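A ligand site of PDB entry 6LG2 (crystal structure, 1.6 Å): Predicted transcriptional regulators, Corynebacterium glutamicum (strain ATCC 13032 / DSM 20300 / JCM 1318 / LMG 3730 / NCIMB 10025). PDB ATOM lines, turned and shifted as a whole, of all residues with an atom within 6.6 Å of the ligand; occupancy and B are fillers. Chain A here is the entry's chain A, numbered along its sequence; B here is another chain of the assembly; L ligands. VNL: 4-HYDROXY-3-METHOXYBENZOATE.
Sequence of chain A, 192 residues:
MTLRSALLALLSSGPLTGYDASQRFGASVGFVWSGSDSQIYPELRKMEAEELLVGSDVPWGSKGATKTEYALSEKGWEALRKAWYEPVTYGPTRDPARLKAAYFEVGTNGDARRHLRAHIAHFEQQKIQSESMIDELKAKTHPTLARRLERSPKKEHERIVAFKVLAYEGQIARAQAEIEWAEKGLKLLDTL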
ATOM      1  N   ALA A   9       9.046  -8.329 -13.473  1.00  0.00           N
ATOM      2  CA  ALA A   9       9.477  -8.931 -12.221  1.00  0.00           C
ATOM      3  C   ALA A   9       8.315  -9.023 -11.226  1.00  0.00           C
ATOM      4  O   ALA A   9       8.111 -10.067 -10.594  1.00  0.00           O
ATOM      5  CB  ALA A   9      10.631  -8.119 -11.639  1.00  0.00           C
ATOM      6  N   LEU A  10       7.554  -7.935 -11.089  1.00  0.00           N
ATOM      7  CA  LEU A  10       6.403  -7.968 -10.183  1.00  0.00           C
ATOM      8  C   LEU A  10       5.393  -9.027 -10.605  1.00  0.00           C
ATOM      9  O   LEU A  10       4.916  -9.815  -9.778  1.00  0.00           O
ATOM     10  CB  LEU A  10       5.729  -6.592 -10.164  1.00  0.00           C
ATOM     11  CG  LEU A  10       4.446  -6.563  -9.328  1.00  0.00           C
ATOM     12  CD1 LEU A  10       4.731  -7.039  -7.882  1.00  0.00           C
ATOM     13  CD2 LEU A  10       3.832  -5.170  -9.335  1.00  0.00           C
ATOM     14  N   SER A  12       5.789 -11.717 -12.243  1.00  0.00           N
ATOM     15  CA  SER A  12       6.193 -13.097 -12.020  1.00  0.00           C
ATOM     16  C   SER A  12       5.770 -13.612 -10.659  1.00  0.00           C
ATOM     17  O   SER A  12       5.837 -14.820 -10.437  1.00  0.00           O
ATOM     18  CB  SER A  12       7.710 -13.256 -12.201  1.00  0.00           C
ATOM     19  OG  SER A  12       8.440 -12.539 -11.216  1.00  0.00           O
ATOM     20  N   SER A  13       5.335 -12.735  -9.748  1.00  0.00           N
ATOM     21  CA  SER A  13       4.788 -13.210  -8.474  1.00  0.00           C
ATOM     22  C   SER A  13       3.340 -13.639  -8.573  1.00  0.00           C
ATOM     23  O   SER A  13       2.794 -14.155  -7.596  1.00  0.00           O
ATOM     24  CB  SER A  13       4.927 -12.136  -7.400  1.00  0.00           C
ATOM     25  OG  SER A  13       3.972 -11.113  -7.595  1.00  0.00           O
ATOM     26  N   ALA A  27       4.380  -0.759  -2.928  1.00  0.00           N
ATOM     27  CA  ALA A  27       4.728  -1.360  -1.650  1.00  0.00           C
ATOM     28  C   ALA A  27       5.875  -2.351  -1.745  1.00  0.00           C
ATOM     29  O   ALA A  27       6.299  -2.880  -0.712  1.00  0.00           O
ATOM     30  CB  ALA A  27       3.496  -2.042  -1.046  1.00  0.00           C
ATOM     31  N   SER A  28       6.409  -2.615  -2.938  1.00  0.00           N
ATOM     32  CA  SER A  28       7.486  -3.596  -3.068  1.00  0.00           C
ATOM     33  C   SER A  28       8.634  -3.058  -3.911  1.00  0.00           C
ATOM     34  O   SER A  28       9.524  -2.364  -3.411  1.00  0.00           O
ATOM     35  CB  SER A  28       6.953  -4.901  -3.666  1.00  0.00           C
ATOM     36  OG  SER A  28       6.309  -4.703  -4.908  1.00  0.00           O
ATOM     37  N   VAL A  29       8.636  -3.396  -5.210  1.00  0.00           N
ATOM     38  CA  VAL A  29       9.738  -3.009  -6.079  1.00  0.00           C
ATOM     39  C   VAL A  29       9.802  -1.498  -6.310  1.00  0.00           C
ATOM     40  O   VAL A  29      10.866  -0.975  -6.666  1.00  0.00           O
ATOM     41  CB  VAL A  29       9.636  -3.806  -7.388  1.00  0.00           C
ATOM     42  CG1 VAL A  29       8.291  -3.569  -8.062  1.00  0.00           C
ATOM     43  CG2 VAL A  29      10.774  -3.480  -8.329  1.00  0.00           C
ATOM     44  N   GLY A  30       8.691  -0.787  -6.081  1.00  0.00           N
ATOM     45  CA  GLY A  30       8.722   0.668  -6.202  1.00  0.00           C
ATOM     46  C   GLY A  30       9.714   1.352  -5.279  1.00  0.00           C
ATOM     47  O   GLY A  30      10.025   2.524  -5.491  1.00  0.00           O
ATOM     48  N   PHE A  31      10.209   0.661  -4.260  1.00  0.00           N
ATOM     49  CA  PHE A  31      11.222   1.250  -3.388  1.00  0.00           C
ATOM     50  C   PHE A  31      12.612   1.235  -4.014  1.00  0.00           C
ATOM     51  O   PHE A  31      13.484   1.977  -3.557  1.00  0.00           O
ATOM     52  CB  PHE A  31      11.236   0.523  -2.043  1.00  0.00           C
ATOM     53  CG  PHE A  31      10.083   0.905  -1.148  1.00  0.00           C
ATOM     54  CD1 PHE A  31      10.002   2.170  -0.586  1.00  0.00           C
ATOM     55  CD2 PHE A  31       9.061   0.001  -0.892  1.00  0.00           C
ATOM     56  CE1 PHE A  31       8.939   2.517   0.233  1.00  0.00           C
ATOM     57  CE2 PHE A  31       8.002   0.337  -0.081  1.00  0.00           C
ATOM     58  CZ  PHE A  31       7.934   1.597   0.481  1.00  0.00           C
ATOM     59  N   VAL A  32      12.857   0.403  -5.027  1.00  0.00           N
ATOM     60  CA  VAL A  32      14.122   0.443  -5.759  1.00  0.00           C
ATOM     61  C   VAL A  32      13.966   0.926  -7.194  1.00  0.00           C
ATOM     62  O   VAL A  32      14.958   1.357  -7.801  1.00  0.00           O
ATOM     63  CB  VAL A  32      14.834  -0.925  -5.721  1.00  0.00           C
ATOM     64  CG1 VAL A  32      14.946  -1.399  -4.260  1.00  0.00           C
ATOM     65  CG2 VAL A  32      14.116  -1.945  -6.579  1.00  0.00           C
ATOM     66  N   MET A 133      11.187  -3.304   6.097  1.00  0.00           N
ATOM     67  CA  MET A 133      10.988  -4.179   4.951  1.00  0.00           C
ATOM     68  C   MET A 133      11.742  -5.494   5.119  1.00  0.00           C
ATOM     69  O   MET A 133      11.186  -6.561   4.851  1.00  0.00           O
ATOM     70  CB  MET A 133      11.440  -3.487   3.669  1.00  0.00           C
ATOM     71  CG  MET A 133      11.396  -4.364   2.440  1.00  0.00           C
ATOM     72  SD  MET A 133       9.698  -4.646   1.925  1.00  0.00           S
ATOM     73  CE  MET A 133       9.240  -3.008   1.352  1.00  0.00           C
ATOM     74  N   LEU A 137      10.221  -9.235   5.000  1.00  0.00           N
ATOM     75  CA  LEU A 137      10.739 -10.221   4.064  1.00  0.00           C
ATOM     76  C   LEU A 137      11.169 -11.495   4.788  1.00  0.00           C
ATOM     77  O   LEU A 137      10.868 -12.611   4.345  1.00  0.00           O
ATOM     78  CB  LEU A 137      11.915  -9.618   3.272  1.00  0.00           C
ATOM     79  CG  LEU A 137      11.562  -8.480   2.309  1.00  0.00           C
ATOM     80  CD1 LEU A 137      12.820  -7.794   1.795  1.00  0.00           C
ATOM     81  CD2 LEU A 137      10.708  -8.962   1.142  1.00  0.00           C
ATOM     82  N   HIS A 142       5.407 -10.288   3.901  1.00  0.00           N
ATOM     83  CA  HIS A 142       5.201  -9.222   2.935  1.00  0.00           C
ATOM     84  C   HIS A 142       4.272  -9.715   1.837  1.00  0.00           C
ATOM     85  O   HIS A 142       4.538 -10.765   1.235  1.00  0.00           O
ATOM     86  CB  HIS A 142       6.526  -8.764   2.322  1.00  0.00           C
ATOM     87  CG  HIS A 142       6.367  -7.604   1.394  1.00  0.00           C
ATOM     88  ND1 HIS A 142       5.824  -7.738   0.125  1.00  0.00           N
ATOM     89  CD2 HIS A 142       6.639  -6.296   1.556  1.00  0.00           C
ATOM     90  CE1 HIS A 142       5.786  -6.545  -0.458  1.00  0.00           C
ATOM     91  NE2 HIS A 142       6.275  -5.661   0.391  1.00  0.00           N
ATOM     92  N   PRO A 143       3.172  -9.010   1.545  1.00  0.00           N
ATOM     93  CA  PRO A 143       2.128  -9.599   0.669  1.00  0.00           C
ATOM     94  C   PRO A 143       2.612 -10.010  -0.709  1.00  0.00           C
ATOM     95  O   PRO A 143       2.148 -11.030  -1.233  1.00  0.00           O
ATOM     96  CB  PRO A 143       1.084  -8.495   0.586  1.00  0.00           C
ATOM     97  CG  PRO A 143       1.249  -7.735   1.866  1.00  0.00           C
ATOM     98  CD  PRO A 143       2.720  -7.761   2.175  1.00  0.00           C
ATOM     99  N   THR A 144       3.509  -9.259  -1.341  1.00  0.00           N
ATOM    100  CA  THR A 144       3.952  -9.691  -2.655  1.00  0.00           C
ATOM    101  C   THR A 144       4.934 -10.857  -2.541  1.00  0.00           C
ATOM    102  O   THR A 144       4.854 -11.811  -3.325  1.00  0.00           O
ATOM    103  CB  THR A 144       4.569  -8.523  -3.418  1.00  0.00           C
ATOM    104  OG1 THR A 144       3.546  -7.555  -3.696  1.00  0.00           O
ATOM    105  CG2 THR A 144       5.178  -9.013  -4.730  1.00  0.00           C
ATOM    106  N   LEU A 145       5.825 -10.825  -1.546  1.00  0.00           N
ATOM    107  CA  LEU A 145       6.720 -11.948  -1.340  1.00  0.00           C
ATOM    108  C   LEU A 145       5.935 -13.210  -1.013  1.00  0.00           C
ATOM    109  O   LEU A 145       6.243 -14.297  -1.515  1.00  0.00           O
ATOM    110  CB  LEU A 145       7.731 -11.647  -0.238  1.00  0.00           C
ATOM    111  CG  LEU A 145       8.621 -12.821   0.153  1.00  0.00           C
ATOM    112  CD1 LEU A 145       9.603 -13.168  -0.973  1.00  0.00           C
ATOM    113  CD2 LEU A 145       9.376 -12.514   1.435  1.00  0.00           C
ATOM    114  N   ALA A 146       4.900 -13.096  -0.167  1.00  0.00           N
ATOM    115  CA  ALA A 146       4.108 -14.266   0.197  1.00  0.00           C
ATOM    116  C   ALA A 146       3.498 -14.916  -1.029  1.00  0.00           C
ATOM    117  O   ALA A 146       3.529 -16.152  -1.164  1.00  0.00           O
ATOM    118  CB  ALA A 146       3.007 -13.856   1.176  1.00  0.00           C
ATOM    119  N   ARG A 148       4.611 -14.648  -4.140  1.00  0.00           N
ATOM    120  CA  ARG A 148       5.734 -15.179  -4.906  1.00  0.00           C
ATOM    121  C   ARG A 148       6.156 -16.547  -4.375  1.00  0.00           C
ATOM    122  O   ARG A 148       6.331 -17.496  -5.142  1.00  0.00           O
ATOM    123  CB  ARG A 148       6.894 -14.197  -4.849  1.00  0.00           C
ATOM    124  CG  ARG A 148       8.136 -14.647  -5.630  1.00  0.00           C
ATOM    125  CD  ARG A 148       9.191 -13.554  -5.667  1.00  0.00           C
ATOM    126  NE  ARG A 148       8.657 -12.310  -6.198  1.00  0.00           N
ATOM    127  CZ  ARG A 148       8.459 -12.072  -7.488  1.00  0.00           C
ATOM    128  NH1 ARG A 148       8.753 -12.985  -8.401  1.00  0.00           N
ATOM    129  NH2 ARG A 148       7.949 -10.904  -7.857  1.00  0.00           N
ATOM    130  N   ILE A 160      15.290 -16.533  -3.131  1.00  0.00           N
ATOM    131  CA  ILE A 160      14.302 -15.486  -3.383  1.00  0.00           C
ATOM    132  C   ILE A 160      14.302 -14.476  -2.244  1.00  0.00           C
ATOM    133  O   ILE A 160      14.406 -13.272  -2.467  1.00  0.00           O
ATOM    134  CB  ILE A 160      12.896 -16.087  -3.603  1.00  0.00           C
ATOM    135  CG1 ILE A 160      12.809 -16.844  -4.917  1.00  0.00           C
ATOM    136  CG2 ILE A 160      11.835 -14.979  -3.628  1.00  0.00           C
ATOM    137  CD1 ILE A 160      11.572 -17.724  -4.971  1.00  0.00           C
ATOM    138  N   LYS A 164      15.936 -10.285  -2.087  1.00  0.00           N
ATOM    139  CA  LYS A 164      15.150  -9.137  -1.653  1.00  0.00           C
ATOM    140  C   LYS A 164      15.822  -8.467  -0.466  1.00  0.00           C
ATOM    141  O   LYS A 164      15.916  -7.227  -0.402  1.00  0.00           O
ATOM    142  CB  LYS A 164      13.721  -9.546  -1.290  1.00  0.00           C
ATOM    143  CG  LYS A 164      13.019 -10.513  -2.216  1.00  0.00           C
ATOM    144  CD  LYS A 164      12.677  -9.898  -3.520  1.00  0.00           C
ATOM    145  CE  LYS A 164      12.300 -10.979  -4.529  1.00  0.00           C
ATOM    146  NZ  LYS A 164      13.516 -11.786  -4.835  1.00  0.00           N
ATOM    147  N   ALA A 167      18.821  -6.437  -1.605  1.00  0.00           N
ATOM    148  CA  ALA A 167      18.498  -5.160  -2.221  1.00  0.00           C
ATOM    149  C   ALA A 167      18.276  -4.088  -1.162  1.00  0.00           C
ATOM    150  O   ALA A 167      18.736  -2.949  -1.304  1.00  0.00           O
ATOM    151  CB  ALA A 167      17.271  -5.302  -3.124  1.00  0.00           C
ATOM    152  N   TYR A 168      17.587  -4.440  -0.070  1.00  0.00           N
ATOM    153  CA  TYR A 168      17.308  -3.448   0.953  1.00  0.00           C
ATOM    154  C   TYR A 168      18.505  -3.185   1.846  1.00  0.00           C
ATOM    155  O   TYR A 168      18.622  -2.081   2.387  1.00  0.00           O
ATOM    156  CB  TYR A 168      16.062  -3.867   1.756  1.00  0.00           C
ATOM    157  CG  TYR A 168      14.825  -3.580   0.937  1.00  0.00           C
ATOM    158  CD1 TYR A 168      14.332  -2.285   0.839  1.00  0.00           C
ATOM    159  CD2 TYR A 168      14.223  -4.578   0.190  1.00  0.00           C
ATOM    160  CE1 TYR A 168      13.245  -1.993   0.054  1.00  0.00           C
ATOM    161  CE2 TYR A 168      13.118  -4.298  -0.614  1.00  0.00           C
ATOM    162  CZ  TYR A 168      12.639  -2.996  -0.665  1.00  0.00           C
ATOM    163  OH  TYR A 168      11.550  -2.691  -1.456  1.00  0.00           O
ATOM    164  N   ARG B  98      20.108  -2.007  -8.068  1.00  0.00           N
ATOM    165  CA  ARG B  98      19.329  -2.500  -6.934  1.00  0.00           C
ATOM    166  C   ARG B  98      18.141  -3.330  -7.430  1.00  0.00           C
ATOM    167  O   ARG B  98      17.820  -4.368  -6.840  1.00  0.00           O
ATOM    168  CB  ARG B  98      18.869  -1.323  -6.072  1.00  0.00           C
ATOM    169  CG  ARG B  98      18.816  -1.604  -4.588  1.00  0.00           C
ATOM    170  CD  ARG B  98      20.206  -1.661  -3.970  1.00  0.00           C
ATOM    171  NE  ARG B  98      20.665  -0.323  -3.598  1.00  0.00           N
ATOM    172  CZ  ARG B  98      21.926   0.076  -3.708  1.00  0.00           C
ATOM    173  NH1 ARG B  98      22.259   1.328  -3.389  1.00  0.00           N
ATOM    174  NH2 ARG B  98      22.856  -0.759  -4.169  1.00  0.00           N
ATOM    175  N   LEU B  99      17.493  -2.887  -8.505  1.00  0.00           N
ATOM    176  CA  LEU B  99      16.409  -3.654  -9.107  1.00  0.00           C
ATOM    177  C   LEU B  99      16.914  -5.006  -9.597  1.00  0.00           C
ATOM    178  O   LEU B  99      16.283  -6.041  -9.362  1.00  0.00           O
ATOM    179  CB  LEU B  99      15.766  -2.870 -10.263  1.00  0.00           C
ATOM    180  CG  LEU B  99      14.774  -3.613 -11.162  1.00  0.00           C
ATOM    181  CD1 LEU B  99      13.547  -4.045 -10.381  1.00  0.00           C
ATOM    182  CD2 LEU B  99      14.409  -2.733 -12.354  1.00  0.00           C
ATOM    183  N   ALA B 102      17.568  -7.291  -6.629  1.00  0.00           N
ATOM    184  CA  ALA B 102      16.362  -7.742  -5.943  1.00  0.00           C
ATOM    185  C   ALA B 102      15.802  -9.021  -6.562  1.00  0.00           C
ATOM    186  O   ALA B 102      15.187  -9.838  -5.873  1.00  0.00           O
ATOM    187  CB  ALA B 102      15.292  -6.639  -5.978  1.00  0.00           C
ATOM    188  N   TYR B 103      16.049  -9.218  -7.850  1.00  0.00           N
ATOM    189  CA  TYR B 103      15.494 -10.355  -8.579  1.00  0.00           C
ATOM    190  C   TYR B 103      16.573 -11.217  -9.201  1.00  0.00           C
ATOM    191  O   TYR B 103      16.378 -11.797 -10.271  1.00  0.00           O
ATOM    192  CB  TYR B 103      14.495  -9.860  -9.636  1.00  0.00           C
ATOM    193  CG  TYR B 103      13.290  -9.182  -9.019  1.00  0.00           C
ATOM    194  CD1 TYR B 103      12.246  -9.937  -8.478  1.00  0.00           C
ATOM    195  CD2 TYR B 103      13.208  -7.806  -8.951  1.00  0.00           C
ATOM    196  CE1 TYR B 103      11.134  -9.303  -7.901  1.00  0.00           C
ATOM    197  CE2 TYR B 103      12.108  -7.176  -8.374  1.00  0.00           C
ATOM    198  CZ  TYR B 103      11.093  -7.938  -7.845  1.00  0.00           C
ATOM    199  OH  TYR B 103       9.994  -7.328  -7.279  1.00  0.00           O
ATOM    200  N   GLU B 105      17.240 -14.067  -8.564  1.00  0.00           N
ATOM    201  CA  GLU B 105      16.775 -15.435  -8.739  1.00  0.00           C
ATOM    202  C   GLU B 105      16.238 -15.695 -10.131  1.00  0.00           C
ATOM    203  O   GLU B 105      16.011 -16.868 -10.481  1.00  0.00           O
ATOM    204  CB  GLU B 105      15.731 -15.777  -7.674  1.00  0.00           C
ATOM    205  CG  GLU B 105      14.349 -15.199  -7.928  1.00  0.00           C
ATOM    206  CD  GLU B 105      14.136 -13.896  -7.187  1.00  0.00           C
ATOM    207  OE1 GLU B 105      15.149 -13.260  -6.813  1.00  0.00           O
ATOM    208  OE2 GLU B 105      12.956 -13.527  -6.964  1.00  0.00           O
HETATM  209  C1  VNL L   1       9.111  -8.286  -3.665  1.00  0.00           C
HETATM  210  CO1 VNL L   1       8.570  -8.279  -2.375  1.00  0.00           C
HETATM  211  CO2 VNL L   1      10.011  -7.279  -4.047  1.00  0.00           C
HETATM  212  CM1 VNL L   1       8.921  -7.291  -1.487  1.00  0.00           C
HETATM  213  CM2 VNL L   1      10.353  -6.292  -3.139  1.00  0.00           C
HETATM  214  OM  VNL L   1      11.222  -5.302  -3.491  1.00  0.00           O
HETATM  215  CZ  VNL L   1       9.807  -6.301  -1.866  1.00  0.00           C
HETATM  216  CC  VNL L   1       8.706  -9.346  -4.587  1.00  0.00           C
HETATM  217  CV  VNL L   1      12.013  -5.475  -4.666  1.00  0.00           C
HETATM  218  O1  VNL L   1       8.415 -10.449  -4.136  1.00  0.00           O
HETATM  219  O2  VNL L   1       8.616  -9.108  -5.799  1.00  0.00           O
HETATM  220  O3  VNL L   1      10.127  -5.334  -0.979  1.00  0.00           O
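O of Ser 28 sits close to OM of the ligand. Residues that only touch the ligand: His 142, Thr 144, Leu 137, Leu 145, Val 29, Ala 102 of chain B and Lys 164. Hydrophobic or aromatic side chains within 4 Å of the ligand: Val 29, Met 133, Leu 137, His 142, Tyr 168, Ala 102 of chain B and Tyr 103 of chain B. Of the 27 residues printed, 12 come within 4 Å of the ligand. The nearest printed residue that does not touch the ligand is Val 32 (4.5 Å).
The side-chain hydroxyl of Tyr 103 of chain B lies within hydrogen-bond range of an oxygen (O2) of the ligand (2.7 Å). The guanidinium group (NE) of Arg 148 lies within salt-bridge range of an oxygen (O1) of the ligand, at 2.8 Å. SD of Met 133 lies within hydrogen-bond range of O3 of the ligand. The side-chain hydroxyl (OH) of Tyr 168 sits at hydrogen-bond distance from an oxygen (O3) of the ligand, 3.0 Å away.
The guanidinium group of Arg 148 is in hydrogen-bond range of the backbone carbonyl oxygen of Ala 9 (2.9 Å). The guanidinium group (NH1) of Arg 148 is in hydrogen-bond range of the side-chain hydroxyl (OG) of Ser 12 (2.9 Å). The backbone carbonyl oxygen (O) of Ser 28 sits at hydrogen-bond distance from the side-chain hydroxyl (OH) of Tyr 168, at 2.8 Å. A ring nitrogen (ND1) of His 142 lies within hydrogen-bond range of the backbone NH (N) of Thr 144. O of Ala 27 lies within hydrogen-bond range of NE2 of His 142 (3.0 Å). O of Ala 102 of chain B sits at hydrogen-bond distance from NZ of Lys 164, 2.8 Å away. The side-chain amino group (NZ) of Lys 164 is in hydrogen-bond range of the backbone carbonyl oxygen (O) of Ile 160 (2.9 Å). The side-chain amino group (NZ) of Lys 164 is in salt-bridge range of the side-chain carboxylate (OE2) of Glu 105 of chain B (2.8 Å).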
